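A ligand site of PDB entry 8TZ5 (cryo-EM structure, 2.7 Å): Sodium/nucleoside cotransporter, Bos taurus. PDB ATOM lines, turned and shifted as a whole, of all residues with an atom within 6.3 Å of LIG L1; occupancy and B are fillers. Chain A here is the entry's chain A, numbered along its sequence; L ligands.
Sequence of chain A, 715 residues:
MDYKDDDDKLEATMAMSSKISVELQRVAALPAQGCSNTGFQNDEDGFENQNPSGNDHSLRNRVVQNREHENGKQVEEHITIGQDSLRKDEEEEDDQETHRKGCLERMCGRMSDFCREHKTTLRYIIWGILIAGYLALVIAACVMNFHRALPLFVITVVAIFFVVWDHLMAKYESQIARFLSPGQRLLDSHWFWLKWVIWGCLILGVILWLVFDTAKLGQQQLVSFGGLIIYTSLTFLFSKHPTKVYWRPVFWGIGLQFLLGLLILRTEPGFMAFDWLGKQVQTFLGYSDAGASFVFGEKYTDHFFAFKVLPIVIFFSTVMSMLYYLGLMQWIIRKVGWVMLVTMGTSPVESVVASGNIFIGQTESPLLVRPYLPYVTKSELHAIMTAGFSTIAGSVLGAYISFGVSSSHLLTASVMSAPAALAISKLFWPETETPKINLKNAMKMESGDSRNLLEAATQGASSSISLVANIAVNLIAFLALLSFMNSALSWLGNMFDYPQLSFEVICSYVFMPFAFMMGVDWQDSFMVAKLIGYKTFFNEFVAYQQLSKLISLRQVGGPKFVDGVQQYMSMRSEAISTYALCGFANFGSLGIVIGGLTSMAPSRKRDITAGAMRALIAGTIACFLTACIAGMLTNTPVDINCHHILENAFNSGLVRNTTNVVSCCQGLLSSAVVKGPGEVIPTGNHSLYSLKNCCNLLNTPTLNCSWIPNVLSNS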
ATOM      1  N   TRP A 191      24.514 -19.111   4.673  1.00  0.00           N
ATOM      2  CA  TRP A 191      24.054 -18.063   3.763  1.00  0.00           C
ATOM      3  C   TRP A 191      24.574 -16.683   4.154  1.00  0.00           C
ATOM      4  O   TRP A 191      24.931 -15.898   3.274  1.00  0.00           O
ATOM      5  CB  TRP A 191      22.521 -18.047   3.722  1.00  0.00           C
ATOM      6  CG  TRP A 191      21.955 -16.870   2.991  1.00  0.00           C
ATOM      7  CD1 TRP A 191      21.371 -15.765   3.542  1.00  0.00           C
ATOM      8  CD2 TRP A 191      21.914 -16.679   1.575  1.00  0.00           C
ATOM      9  NE1 TRP A 191      20.970 -14.901   2.552  1.00  0.00           N
ATOM     10  CE2 TRP A 191      21.294 -15.437   1.335  1.00  0.00           C
ATOM     11  CE3 TRP A 191      22.352 -17.436   0.475  1.00  0.00           C
ATOM     12  CZ2 TRP A 191      21.090 -14.945   0.053  1.00  0.00           C
ATOM     13  CZ3 TRP A 191      22.155 -16.942  -0.795  1.00  0.00           C
ATOM     14  CH2 TRP A 191      21.523 -15.712  -0.996  1.00  0.00           C
ATOM     15  N   LYS A 195      26.089 -15.352   0.653  1.00  0.00           N
ATOM     16  CA  LYS A 195      25.294 -14.477  -0.198  1.00  0.00           C
ATOM     17  C   LYS A 195      26.160 -13.444  -0.904  1.00  0.00           C
ATOM     18  O   LYS A 195      25.967 -13.160  -2.084  1.00  0.00           O
ATOM     19  CB  LYS A 195      24.204 -13.791   0.622  1.00  0.00           C
ATOM     20  CG  LYS A 195      24.702 -12.705   1.557  1.00  0.00           C
ATOM     21  CD  LYS A 195      23.573 -12.116   2.381  1.00  0.00           C
ATOM     22  CE  LYS A 195      24.033 -10.889   3.138  1.00  0.00           C
ATOM     23  NZ  LYS A 195      22.928 -10.286   3.950  1.00  0.00           N
ATOM     24  N   ILE A 198      28.018 -15.122  -3.775  1.00  0.00           N
ATOM     25  CA  ILE A 198      27.155 -15.410  -4.907  1.00  0.00           C
ATOM     26  C   ILE A 198      26.815 -14.126  -5.663  1.00  0.00           C
ATOM     27  O   ILE A 198      26.845 -14.092  -6.900  1.00  0.00           O
ATOM     28  CB  ILE A 198      25.885 -16.150  -4.447  1.00  0.00           C
ATOM     29  CG1 ILE A 198      26.254 -17.526  -3.885  1.00  0.00           C
ATOM     30  CG2 ILE A 198      24.893 -16.278  -5.597  1.00  0.00           C
ATOM     31  CD1 ILE A 198      25.089 -18.286  -3.284  1.00  0.00           C
ATOM     32  N   TRP A 199      26.475 -13.058  -4.933  1.00  0.00           N
ATOM     33  CA  TRP A 199      26.126 -11.804  -5.586  1.00  0.00           C
ATOM     34  C   TRP A 199      27.304 -11.228  -6.348  1.00  0.00           C
ATOM     35  O   TRP A 199      27.147 -10.714  -7.466  1.00  0.00           O
ATOM     36  CB  TRP A 199      25.612 -10.806  -4.537  1.00  0.00           C
ATOM     37  CG  TRP A 199      24.361 -11.264  -3.840  1.00  0.00           C
ATOM     38  CD1 TRP A 199      23.566 -12.312  -4.188  1.00  0.00           C
ATOM     39  CD2 TRP A 199      23.768 -10.681  -2.672  1.00  0.00           C
ATOM     40  NE1 TRP A 199      22.519 -12.428  -3.315  1.00  0.00           N
ATOM     41  CE2 TRP A 199      22.621 -11.436  -2.371  1.00  0.00           C
ATOM     42  CE3 TRP A 199      24.104  -9.604  -1.856  1.00  0.00           C
ATOM     43  CZ2 TRP A 199      21.795 -11.136  -1.292  1.00  0.00           C
ATOM     44  CZ3 TRP A 199      23.279  -9.304  -0.777  1.00  0.00           C
ATOM     45  CH2 TRP A 199      22.145 -10.078  -0.504  1.00  0.00           C
ATOM     46  N   LEU A 202      27.706 -13.149  -9.569  1.00  0.00           N
ATOM     47  CA  LEU A 202      26.707 -12.746 -10.558  1.00  0.00           C
ATOM     48  C   LEU A 202      27.046 -11.390 -11.172  1.00  0.00           C
ATOM     49  O   LEU A 202      26.927 -11.207 -12.392  1.00  0.00           O
ATOM     50  CB  LEU A 202      25.321 -12.720  -9.923  1.00  0.00           C
ATOM     51  CG  LEU A 202      24.789 -14.081  -9.461  1.00  0.00           C
ATOM     52  CD1 LEU A 202      23.568 -13.900  -8.574  1.00  0.00           C
ATOM     53  CD2 LEU A 202      24.474 -14.971 -10.644  1.00  0.00           C
ATOM     54  N   GLY A 205      29.875 -11.755 -13.562  1.00  0.00           N
ATOM     55  CA  GLY A 205      29.401 -12.348 -14.801  1.00  0.00           C
ATOM     56  C   GLY A 205      28.680 -11.351 -15.676  1.00  0.00           C
ATOM     57  O   GLY A 205      28.869 -11.331 -16.901  1.00  0.00           O
ATOM     58  N   VAL A 206      27.854 -10.496 -15.078  1.00  0.00           N
ATOM     59  CA  VAL A 206      27.156  -9.473 -15.848  1.00  0.00           C
ATOM     60  C   VAL A 206      28.167  -8.526 -16.497  1.00  0.00           C
ATOM     61  O   VAL A 206      28.052  -8.189 -17.680  1.00  0.00           O
ATOM     62  CB  VAL A 206      26.166  -8.698 -14.959  1.00  0.00           C
ATOM     63  CG1 VAL A 206      25.644  -7.473 -15.684  1.00  0.00           C
ATOM     64  CG2 VAL A 206      25.018  -9.591 -14.526  1.00  0.00           C
ATOM     65  N   ILE A 207      29.165  -8.093 -15.727  1.00  0.00           N
ATOM     66  CA  ILE A 207      30.151  -7.158 -16.268  1.00  0.00           C
ATOM     67  C   ILE A 207      30.936  -7.800 -17.404  1.00  0.00           C
ATOM     68  O   ILE A 207      31.182  -7.168 -18.442  1.00  0.00           O
ATOM     69  CB  ILE A 207      31.078  -6.667 -15.140  1.00  0.00           C
ATOM     70  CG1 ILE A 207      30.294  -5.805 -14.146  1.00  0.00           C
ATOM     71  CG2 ILE A 207      32.250  -5.885 -15.739  1.00  0.00           C
ATOM     72  CD1 ILE A 207      31.072  -5.426 -12.903  1.00  0.00           C
ATOM     73  N   TRP A 209      29.992 -10.321 -19.372  1.00  0.00           N
ATOM     74  CA  TRP A 209      29.124 -10.459 -20.533  1.00  0.00           C
ATOM     75  C   TRP A 209      28.984  -9.142 -21.261  1.00  0.00           C
ATOM     76  O   TRP A 209      29.134  -9.077 -22.487  1.00  0.00           O
ATOM     77  CB  TRP A 209      27.757 -10.992 -20.110  1.00  0.00           C
ATOM     78  CG  TRP A 209      26.815 -11.132 -21.275  1.00  0.00           C
ATOM     79  CD1 TRP A 209      25.883 -10.229 -21.686  1.00  0.00           C
ATOM     80  CD2 TRP A 209      26.727 -12.253 -22.166  1.00  0.00           C
ATOM     81  NE1 TRP A 209      25.215 -10.718 -22.788  1.00  0.00           N
ATOM     82  CE2 TRP A 209      25.718 -11.952 -23.108  1.00  0.00           C
ATOM     83  CE3 TRP A 209      27.401 -13.464 -22.277  1.00  0.00           C
ATOM     84  CZ2 TRP A 209      25.364 -12.825 -24.124  1.00  0.00           C
ATOM     85  CZ3 TRP A 209      27.055 -14.335 -23.290  1.00  0.00           C
ATOM     86  CH2 TRP A 209      26.043 -14.014 -24.201  1.00  0.00           C
ATOM     87  N   TYR A 246      10.236  -5.539  -2.124  1.00  0.00           N
ATOM     88  CA  TYR A 246      10.913  -6.825  -2.025  1.00  0.00           C
ATOM     89  C   TYR A 246      11.667  -7.041  -3.337  1.00  0.00           C
ATOM     90  O   TYR A 246      11.045  -7.228  -4.383  1.00  0.00           O
ATOM     91  CB  TYR A 246       9.911  -7.942  -1.748  1.00  0.00           C
ATOM     92  CG  TYR A 246      10.516  -9.295  -1.411  1.00  0.00           C
ATOM     93  CD1 TYR A 246      11.791  -9.391  -0.869  1.00  0.00           C
ATOM     94  CD2 TYR A 246       9.803 -10.459  -1.629  1.00  0.00           C
ATOM     95  CE1 TYR A 246      12.342 -10.622  -0.558  1.00  0.00           C
ATOM     96  CE2 TYR A 246      10.344 -11.692  -1.321  1.00  0.00           C
ATOM     97  CZ  TYR A 246      11.606 -11.769  -0.783  1.00  0.00           C
ATOM     98  OH  TYR A 246      12.147 -13.002  -0.475  1.00  0.00           O
ATOM     99  N   TRP A 247      12.992  -7.019  -3.271  1.00  0.00           N
ATOM    100  CA  TRP A 247      13.817  -6.987  -4.478  1.00  0.00           C
ATOM    101  C   TRP A 247      14.112  -8.362  -5.053  1.00  0.00           C
ATOM    102  O   TRP A 247      14.663  -8.453  -6.157  1.00  0.00           O
ATOM    103  CB  TRP A 247      15.149  -6.289  -4.177  1.00  0.00           C
ATOM    104  CG  TRP A 247      15.025  -4.817  -4.048  1.00  0.00           C
ATOM    105  CD1 TRP A 247      14.958  -4.099  -2.885  1.00  0.00           C
ATOM    106  CD2 TRP A 247      14.957  -3.861  -5.111  1.00  0.00           C
ATOM    107  NE1 TRP A 247      14.847  -2.756  -3.158  1.00  0.00           N
ATOM    108  CE2 TRP A 247      14.845  -2.588  -4.518  1.00  0.00           C
ATOM    109  CE3 TRP A 247      14.979  -3.964  -6.504  1.00  0.00           C
ATOM    110  CZ2 TRP A 247      14.762  -1.425  -5.274  1.00  0.00           C
ATOM    111  CZ3 TRP A 247      14.883  -2.802  -7.253  1.00  0.00           C
ATOM    112  CH2 TRP A 247      14.777  -1.547  -6.637  1.00  0.00           C
ATOM    113  N   ARG A 248      13.769  -9.444  -4.347  1.00  0.00           N
ATOM    114  CA  ARG A 248      14.005 -10.777  -4.899  1.00  0.00           C
ATOM    115  C   ARG A 248      13.233 -11.004  -6.199  1.00  0.00           C
ATOM    116  O   ARG A 248      13.876 -11.392  -7.205  1.00  0.00           O
ATOM    117  CB  ARG A 248      13.631 -11.824  -3.843  1.00  0.00           C
ATOM    118  CG  ARG A 248      13.813 -13.264  -4.279  1.00  0.00           C
ATOM    119  CD  ARG A 248      13.166 -14.225  -3.283  1.00  0.00           C
ATOM    120  NE  ARG A 248      13.358 -15.612  -3.650  1.00  0.00           N
ATOM    121  CZ  ARG A 248      12.722 -16.632  -3.086  1.00  0.00           C
ATOM    122  NH1 ARG A 248      11.836 -16.446  -2.116  1.00  0.00           N
ATOM    123  NH2 ARG A 248      12.970 -17.869  -3.504  1.00  0.00           N
ATOM    124  N   PHE A 251      14.778  -8.922  -9.444  1.00  0.00           N
ATOM    125  CA  PHE A 251      16.015  -9.466  -9.986  1.00  0.00           C
ATOM    126  C   PHE A 251      15.801 -10.843 -10.578  1.00  0.00           C
ATOM    127  O   PHE A 251      16.364 -11.164 -11.632  1.00  0.00           O
ATOM    128  CB  PHE A 251      17.085  -9.500  -8.888  1.00  0.00           C
ATOM    129  CG  PHE A 251      17.609  -8.150  -8.497  1.00  0.00           C
ATOM    130  CD1 PHE A 251      18.025  -7.245  -9.447  1.00  0.00           C
ATOM    131  CD2 PHE A 251      17.667  -7.782  -7.153  1.00  0.00           C
ATOM    132  CE1 PHE A 251      18.503  -6.004  -9.086  1.00  0.00           C
ATOM    133  CE2 PHE A 251      18.145  -6.542  -6.792  1.00  0.00           C
ATOM    134  CZ  PHE A 251      18.556  -5.648  -7.755  1.00  0.00           C
ATOM    135  N   TRP A 252      14.983 -11.677  -9.923  1.00  0.00           N
ATOM    136  CA  TRP A 252      14.780 -13.030 -10.436  1.00  0.00           C
ATOM    137  C   TRP A 252      14.019 -13.003 -11.767  1.00  0.00           C
ATOM    138  O   TRP A 252      14.338 -13.775 -12.674  1.00  0.00           O
ATOM    139  CB  TRP A 252      14.051 -13.881  -9.412  1.00  0.00           C
ATOM    140  CG  TRP A 252      14.975 -14.777  -8.644  1.00  0.00           C
ATOM    141  CD1 TRP A 252      15.321 -14.668  -7.325  1.00  0.00           C
ATOM    142  CD2 TRP A 252      15.689 -15.911  -9.152  1.00  0.00           C
ATOM    143  NE1 TRP A 252      16.197 -15.674  -6.980  1.00  0.00           N
ATOM    144  CE2 TRP A 252      16.437 -16.453  -8.085  1.00  0.00           C
ATOM    145  CE3 TRP A 252      15.760 -16.529 -10.406  1.00  0.00           C
ATOM    146  CZ2 TRP A 252      17.247 -17.573  -8.231  1.00  0.00           C
ATOM    147  CZ3 TRP A 252      16.570 -17.648 -10.552  1.00  0.00           C
ATOM    148  CH2 TRP A 252      17.296 -18.153  -9.470  1.00  0.00           C
ATOM    149  N   ILE A 254      14.006 -10.467 -14.001  1.00  0.00           N
ATOM    150  CA  ILE A 254      14.922  -9.960 -15.024  1.00  0.00           C
ATOM    151  C   ILE A 254      15.912 -11.047 -15.425  1.00  0.00           C
ATOM    152  O   ILE A 254      16.234 -11.217 -16.599  1.00  0.00           O
ATOM    153  CB  ILE A 254      15.636  -8.698 -14.517  1.00  0.00           C
ATOM    154  CG1 ILE A 254      14.628  -7.568 -14.301  1.00  0.00           C
ATOM    155  CG2 ILE A 254      16.737  -8.292 -15.500  1.00  0.00           C
ATOM    156  CD1 ILE A 254      15.224  -6.293 -13.739  1.00  0.00           C
ATOM    157  N   GLY A 255      16.414 -11.803 -14.438  1.00  0.00           N
ATOM    158  CA  GLY A 255      17.344 -12.867 -14.743  1.00  0.00           C
ATOM    159  C   GLY A 255      16.723 -13.990 -15.552  1.00  0.00           C
ATOM    160  O   GLY A 255      17.367 -14.547 -16.447  1.00  0.00           O
ATOM    161  N   LEU A 256      15.484 -14.353 -15.239  1.00  0.00           N
ATOM    162  CA  LEU A 256      14.794 -15.366 -16.026  1.00  0.00           C
ATOM    163  C   LEU A 256      14.597 -14.896 -17.466  1.00  0.00           C
ATOM    164  O   LEU A 256      14.759 -15.684 -18.408  1.00  0.00           O
ATOM    165  CB  LEU A 256      13.452 -15.728 -15.389  1.00  0.00           C
ATOM    166  CG  LEU A 256      13.509 -16.506 -14.070  1.00  0.00           C
ATOM    167  CD1 LEU A 256      12.114 -16.676 -13.498  1.00  0.00           C
ATOM    168  CD2 LEU A 256      14.181 -17.862 -14.261  1.00  0.00           C
ATOM    169  N   PHE A 258      16.564 -12.806 -19.042  1.00  0.00           N
ATOM    170  CA  PHE A 258      17.876 -12.854 -19.670  1.00  0.00           C
ATOM    171  C   PHE A 258      18.270 -14.279 -20.043  1.00  0.00           C
ATOM    172  O   PHE A 258      18.837 -14.529 -21.115  1.00  0.00           O
ATOM    173  CB  PHE A 258      18.929 -12.236 -18.748  1.00  0.00           C
ATOM    174  CG  PHE A 258      20.264 -12.068 -19.394  1.00  0.00           C
ATOM    175  CD1 PHE A 258      20.454 -11.130 -20.390  1.00  0.00           C
ATOM    176  CD2 PHE A 258      21.346 -12.826 -18.991  1.00  0.00           C
ATOM    177  CE1 PHE A 258      21.677 -10.969 -20.990  1.00  0.00           C
ATOM    178  CE2 PHE A 258      22.577 -12.673 -19.578  1.00  0.00           C
ATOM    179  CZ  PHE A 258      22.748 -11.738 -20.580  1.00  0.00           C
ATOM    180  N   LEU A 259      17.974 -15.247 -19.159  1.00  0.00           N
ATOM    181  CA  LEU A 259      18.301 -16.640 -19.449  1.00  0.00           C
ATOM    182  C   LEU A 259      17.480 -17.156 -20.625  1.00  0.00           C
ATOM    183  O   LEU A 259      18.021 -17.871 -21.487  1.00  0.00           O
ATOM    184  CB  LEU A 259      18.043 -17.491 -18.209  1.00  0.00           C
ATOM    185  CG  LEU A 259      18.980 -17.240 -17.021  1.00  0.00           C
ATOM    186  CD1 LEU A 259      18.540 -18.071 -15.822  1.00  0.00           C
ATOM    187  CD2 LEU A 259      20.417 -17.545 -17.392  1.00  0.00           C
ATOM    188  N   LEU A 262      19.027 -15.709 -23.752  1.00  0.00           N
ATOM    189  CA  LEU A 262      20.266 -16.420 -24.097  1.00  0.00           C
ATOM    190  C   LEU A 262      19.953 -17.773 -24.723  1.00  0.00           C
ATOM    191  O   LEU A 262      20.546 -18.148 -25.747  1.00  0.00           O
ATOM    192  CB  LEU A 262      21.127 -16.595 -22.854  1.00  0.00           C
ATOM    193  CG  LEU A 262      21.816 -15.346 -22.303  1.00  0.00           C
ATOM    194  CD1 LEU A 262      22.552 -15.682 -21.022  1.00  0.00           C
ATOM    195  CD2 LEU A 262      22.762 -14.763 -23.324  1.00  0.00           C
HETATM  196  C1  LIG L   1      17.470 -14.520  -0.601  1.00  0.00           C
HETATM  197  P1  LIG L   1      15.099 -14.154   0.508  1.00  0.00           P
HETATM  198  C2  LIG L   1      18.071 -14.458  -2.011  1.00  0.00           C
HETATM  199  C3  LIG L   1      18.018 -15.831  -2.664  1.00  0.00           C
HETATM  200  C4  LIG L   1      19.399 -15.073 -12.863  1.00  0.00           C
HETATM  201  O1  LIG L   1      16.073 -14.727  -0.708  1.00  0.00           O
HETATM  202  C5  LIG L   1      20.916 -15.289 -13.013  1.00  0.00           C
HETATM  203  O2  LIG L   1      14.946 -12.652   0.374  1.00  0.00           O
HETATM  204  C6  LIG L   1      21.361 -14.858 -14.434  1.00  0.00           C
HETATM  205  O3  LIG L   1      13.738 -14.800   0.421  1.00  0.00           O
HETATM  206  C7  LIG L   1      22.691 -14.086 -14.407  1.00  0.00           C
HETATM  207  O4  LIG L   1      15.775 -14.505   1.968  1.00  0.00           O
HETATM  208  C8  LIG L   1      23.191 -13.737 -15.821  1.00  0.00           C
HETATM  209  C9  LIG L   1      24.690 -13.435 -15.835  1.00  0.00           C
HETATM  210  C10 LIG L   1      25.124 -12.646 -17.058  1.00  0.00           C
HETATM  211  C11 LIG L   1      25.976 -13.436 -18.037  1.00  0.00           C
HETATM  212  C12 LIG L   1      25.407 -14.792 -18.391  1.00  0.00           C
HETATM  213  C13 LIG L   1      19.960 -15.806  -4.025  1.00  0.00           C
HETATM  214  O5  LIG L   1      19.334 -16.293  -2.859  1.00  0.00           O
HETATM  215  C14 LIG L   1      19.962 -16.628  -5.319  1.00  0.00           C
HETATM  216  O6  LIG L   1      20.481 -14.749  -4.003  1.00  0.00           O
HETATM  217  C15 LIG L   1      21.348 -17.194  -5.663  1.00  0.00           C
HETATM  218  C16 LIG L   1      21.324 -18.051  -6.956  1.00  0.00           C
HETATM  219  C17 LIG L   1      22.037 -17.367  -8.129  1.00  0.00           C
HETATM  220  C18 LIG L   1      22.342 -18.350  -9.260  1.00  0.00           C
HETATM  221  C19 LIG L   1      21.696 -17.930 -10.592  1.00  0.00           C
HETATM  222  C20 LIG L   1      17.720 -12.179  -2.602  1.00  0.00           C
HETATM  223  O7  LIG L   1      17.343 -13.541  -2.795  1.00  0.00           O
HETATM  224  C21 LIG L   1      18.797 -11.543  -3.534  1.00  0.00           C
HETATM  225  O8  LIG L   1      17.223 -11.538  -1.738  1.00  0.00           O
HETATM  226  C22 LIG L   1      18.358 -11.519  -5.018  1.00  0.00           C
HETATM  227  C23 LIG L   1      19.235 -12.433  -5.886  1.00  0.00           C
HETATM  228  C24 LIG L   1      18.827 -12.424  -7.360  1.00  0.00           C
HETATM  229  C25 LIG L   1      19.176 -13.733  -8.063  1.00  0.00           C
HETATM  230  C26 LIG L   1      19.274 -13.583  -9.580  1.00  0.00           C
HETATM  231  C27 LIG L   1      19.531 -14.927 -10.305  1.00  0.00           C
HETATM  232  C28 LIG L   1      18.780 -14.910 -11.664  1.00  0.00           C
HETATM  233  C1  LG2 L   2      17.438  -5.300   0.420  1.00  0.00           C
HETATM  234  P1  LG2 L   2      15.468  -7.089   0.692  1.00  0.00           P
HETATM  235  C2  LG2 L   2      17.835  -5.697  -1.010  1.00  0.00           C
HETATM  236  C3  LG2 L   2      18.672  -4.606  -1.630  1.00  0.00           C
HETATM  237  C4  LG2 L   2      21.546  -9.213 -10.706  1.00  0.00           C
HETATM  238  O1  LG2 L   2      16.957  -6.455   1.098  1.00  0.00           O
HETATM  239  C5  LG2 L   2      20.668 -10.399 -11.150  1.00  0.00           C
HETATM  240  O2  LG2 L   2      15.483  -7.558  -0.746  1.00  0.00           O
HETATM  241  C6  LG2 L   2      19.941 -10.032 -12.469  1.00  0.00           C
HETATM  242  O3  LG2 L   2      14.396  -6.031   0.852  1.00  0.00           O
HETATM  243  C7  LG2 L   2      20.755 -10.448 -13.704  1.00  0.00           C
HETATM  244  O4  LG2 L   2      15.133  -8.354   1.681  1.00  0.00           O
HETATM  245  C8  LG2 L   2      20.187  -9.853 -15.004  1.00  0.00           C
HETATM  246  C9  LG2 L   2      21.269  -9.563 -16.029  1.00  0.00           C
HETATM  247  C10 LG2 L   2      20.715  -8.903 -17.280  1.00  0.00           C
HETATM  248  C11 LG2 L   2      21.779  -8.309 -18.186  1.00  0.00           C
HETATM  249  C12 LG2 L   2      23.104  -9.046 -18.121  1.00  0.00           C
HETATM  250  C13 LG2 L   2      18.557  -2.797  -3.128  1.00  0.00           C
HETATM  251  O5  LG2 L   2      17.871  -3.854  -2.497  1.00  0.00           O
HETATM  252  C14 LG2 L   2      19.609  -3.111  -4.204  1.00  0.00           C
HETATM  253  O6  LG2 L   2      18.327  -1.672  -2.834  1.00  0.00           O
HETATM  254  C15 LG2 L   2      19.366  -2.332  -5.512  1.00  0.00           C
HETATM  255  C16 LG2 L   2      20.676  -1.987  -6.235  1.00  0.00           C
HETATM  256  C17 LG2 L   2      21.362  -3.239  -6.820  1.00  0.00           C
HETATM  257  C18 LG2 L   2      21.647  -3.099  -8.315  1.00  0.00           C
HETATM  258  C19 LG2 L   2      22.487  -4.264  -8.865  1.00  0.00           C
HETATM  259  C20 LG2 L   2      18.301  -7.806  -2.025  1.00  0.00           C
HETATM  260  O7  LG2 L   2      18.592  -6.902  -0.966  1.00  0.00           O
HETATM  261  C21 LG2 L   2      19.014  -7.645  -3.404  1.00  0.00           C
HETATM  262  O8  LG2 L   2      17.515  -8.688  -1.868  1.00  0.00           O
HETATM  263  C22 LG2 L   2      20.557  -7.707  -3.276  1.00  0.00           C
HETATM  264  C23 LG2 L   2      21.232  -7.714  -4.652  1.00  0.00           C
HETATM  265  C24 LG2 L   2      21.632  -9.130  -5.107  1.00  0.00           C
HETATM  266  C25 LG2 L   2      21.508  -9.290  -6.637  1.00  0.00           C
HETATM  267  C26 LG2 L   2      22.634 -10.137  -7.237  1.00  0.00           C
HETATM  268  C27 LG2 L   2      22.302 -10.541  -8.697  1.00  0.00           C
HETATM  269  C28 LG2 L   2      22.290  -9.278  -9.583  1.00  0.00           C
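The side-chain hydroxyl (OH) of Tyr 246 sits at hydrogen-bond distance from an oxygen (O3) of LIG L1 (2.6 Å).
NE1 of Trp 199 sits at hydrogen-bond distance from O6 of LIG L1 (3.2 Å).
NH1 of Arg 248 is in salt-bridge range of O3 of LIG L1 (3.6 Å).
An oxygen (O5) of LG2 L2 sits close to the indole nitrogen of Trp 247, at 3.3 Å.
Residues that only touch LIG L1: Trp 191 (2.9 Å), Gly 255 (3.6 Å), Phe 258 (3.6 Å), Trp 252 (3.7 Å), Ile 198 (3.7 Å), Trp 209 (3.7 Å), Phe 251 (3.7 Å), Gly 205 (3.8 Å), Leu 202 (3.8 Å), Val 206 (3.96 Å) and Leu 262 (3.98 Å).
Hydrophobic or aromatic side chains within 4 Å of LIG L1: Trp 191, Ile 198, Trp 199, Leu 202, Val 206, Trp 209, Tyr 246, Phe 251, Trp 252, Phe 258 and Leu 262.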
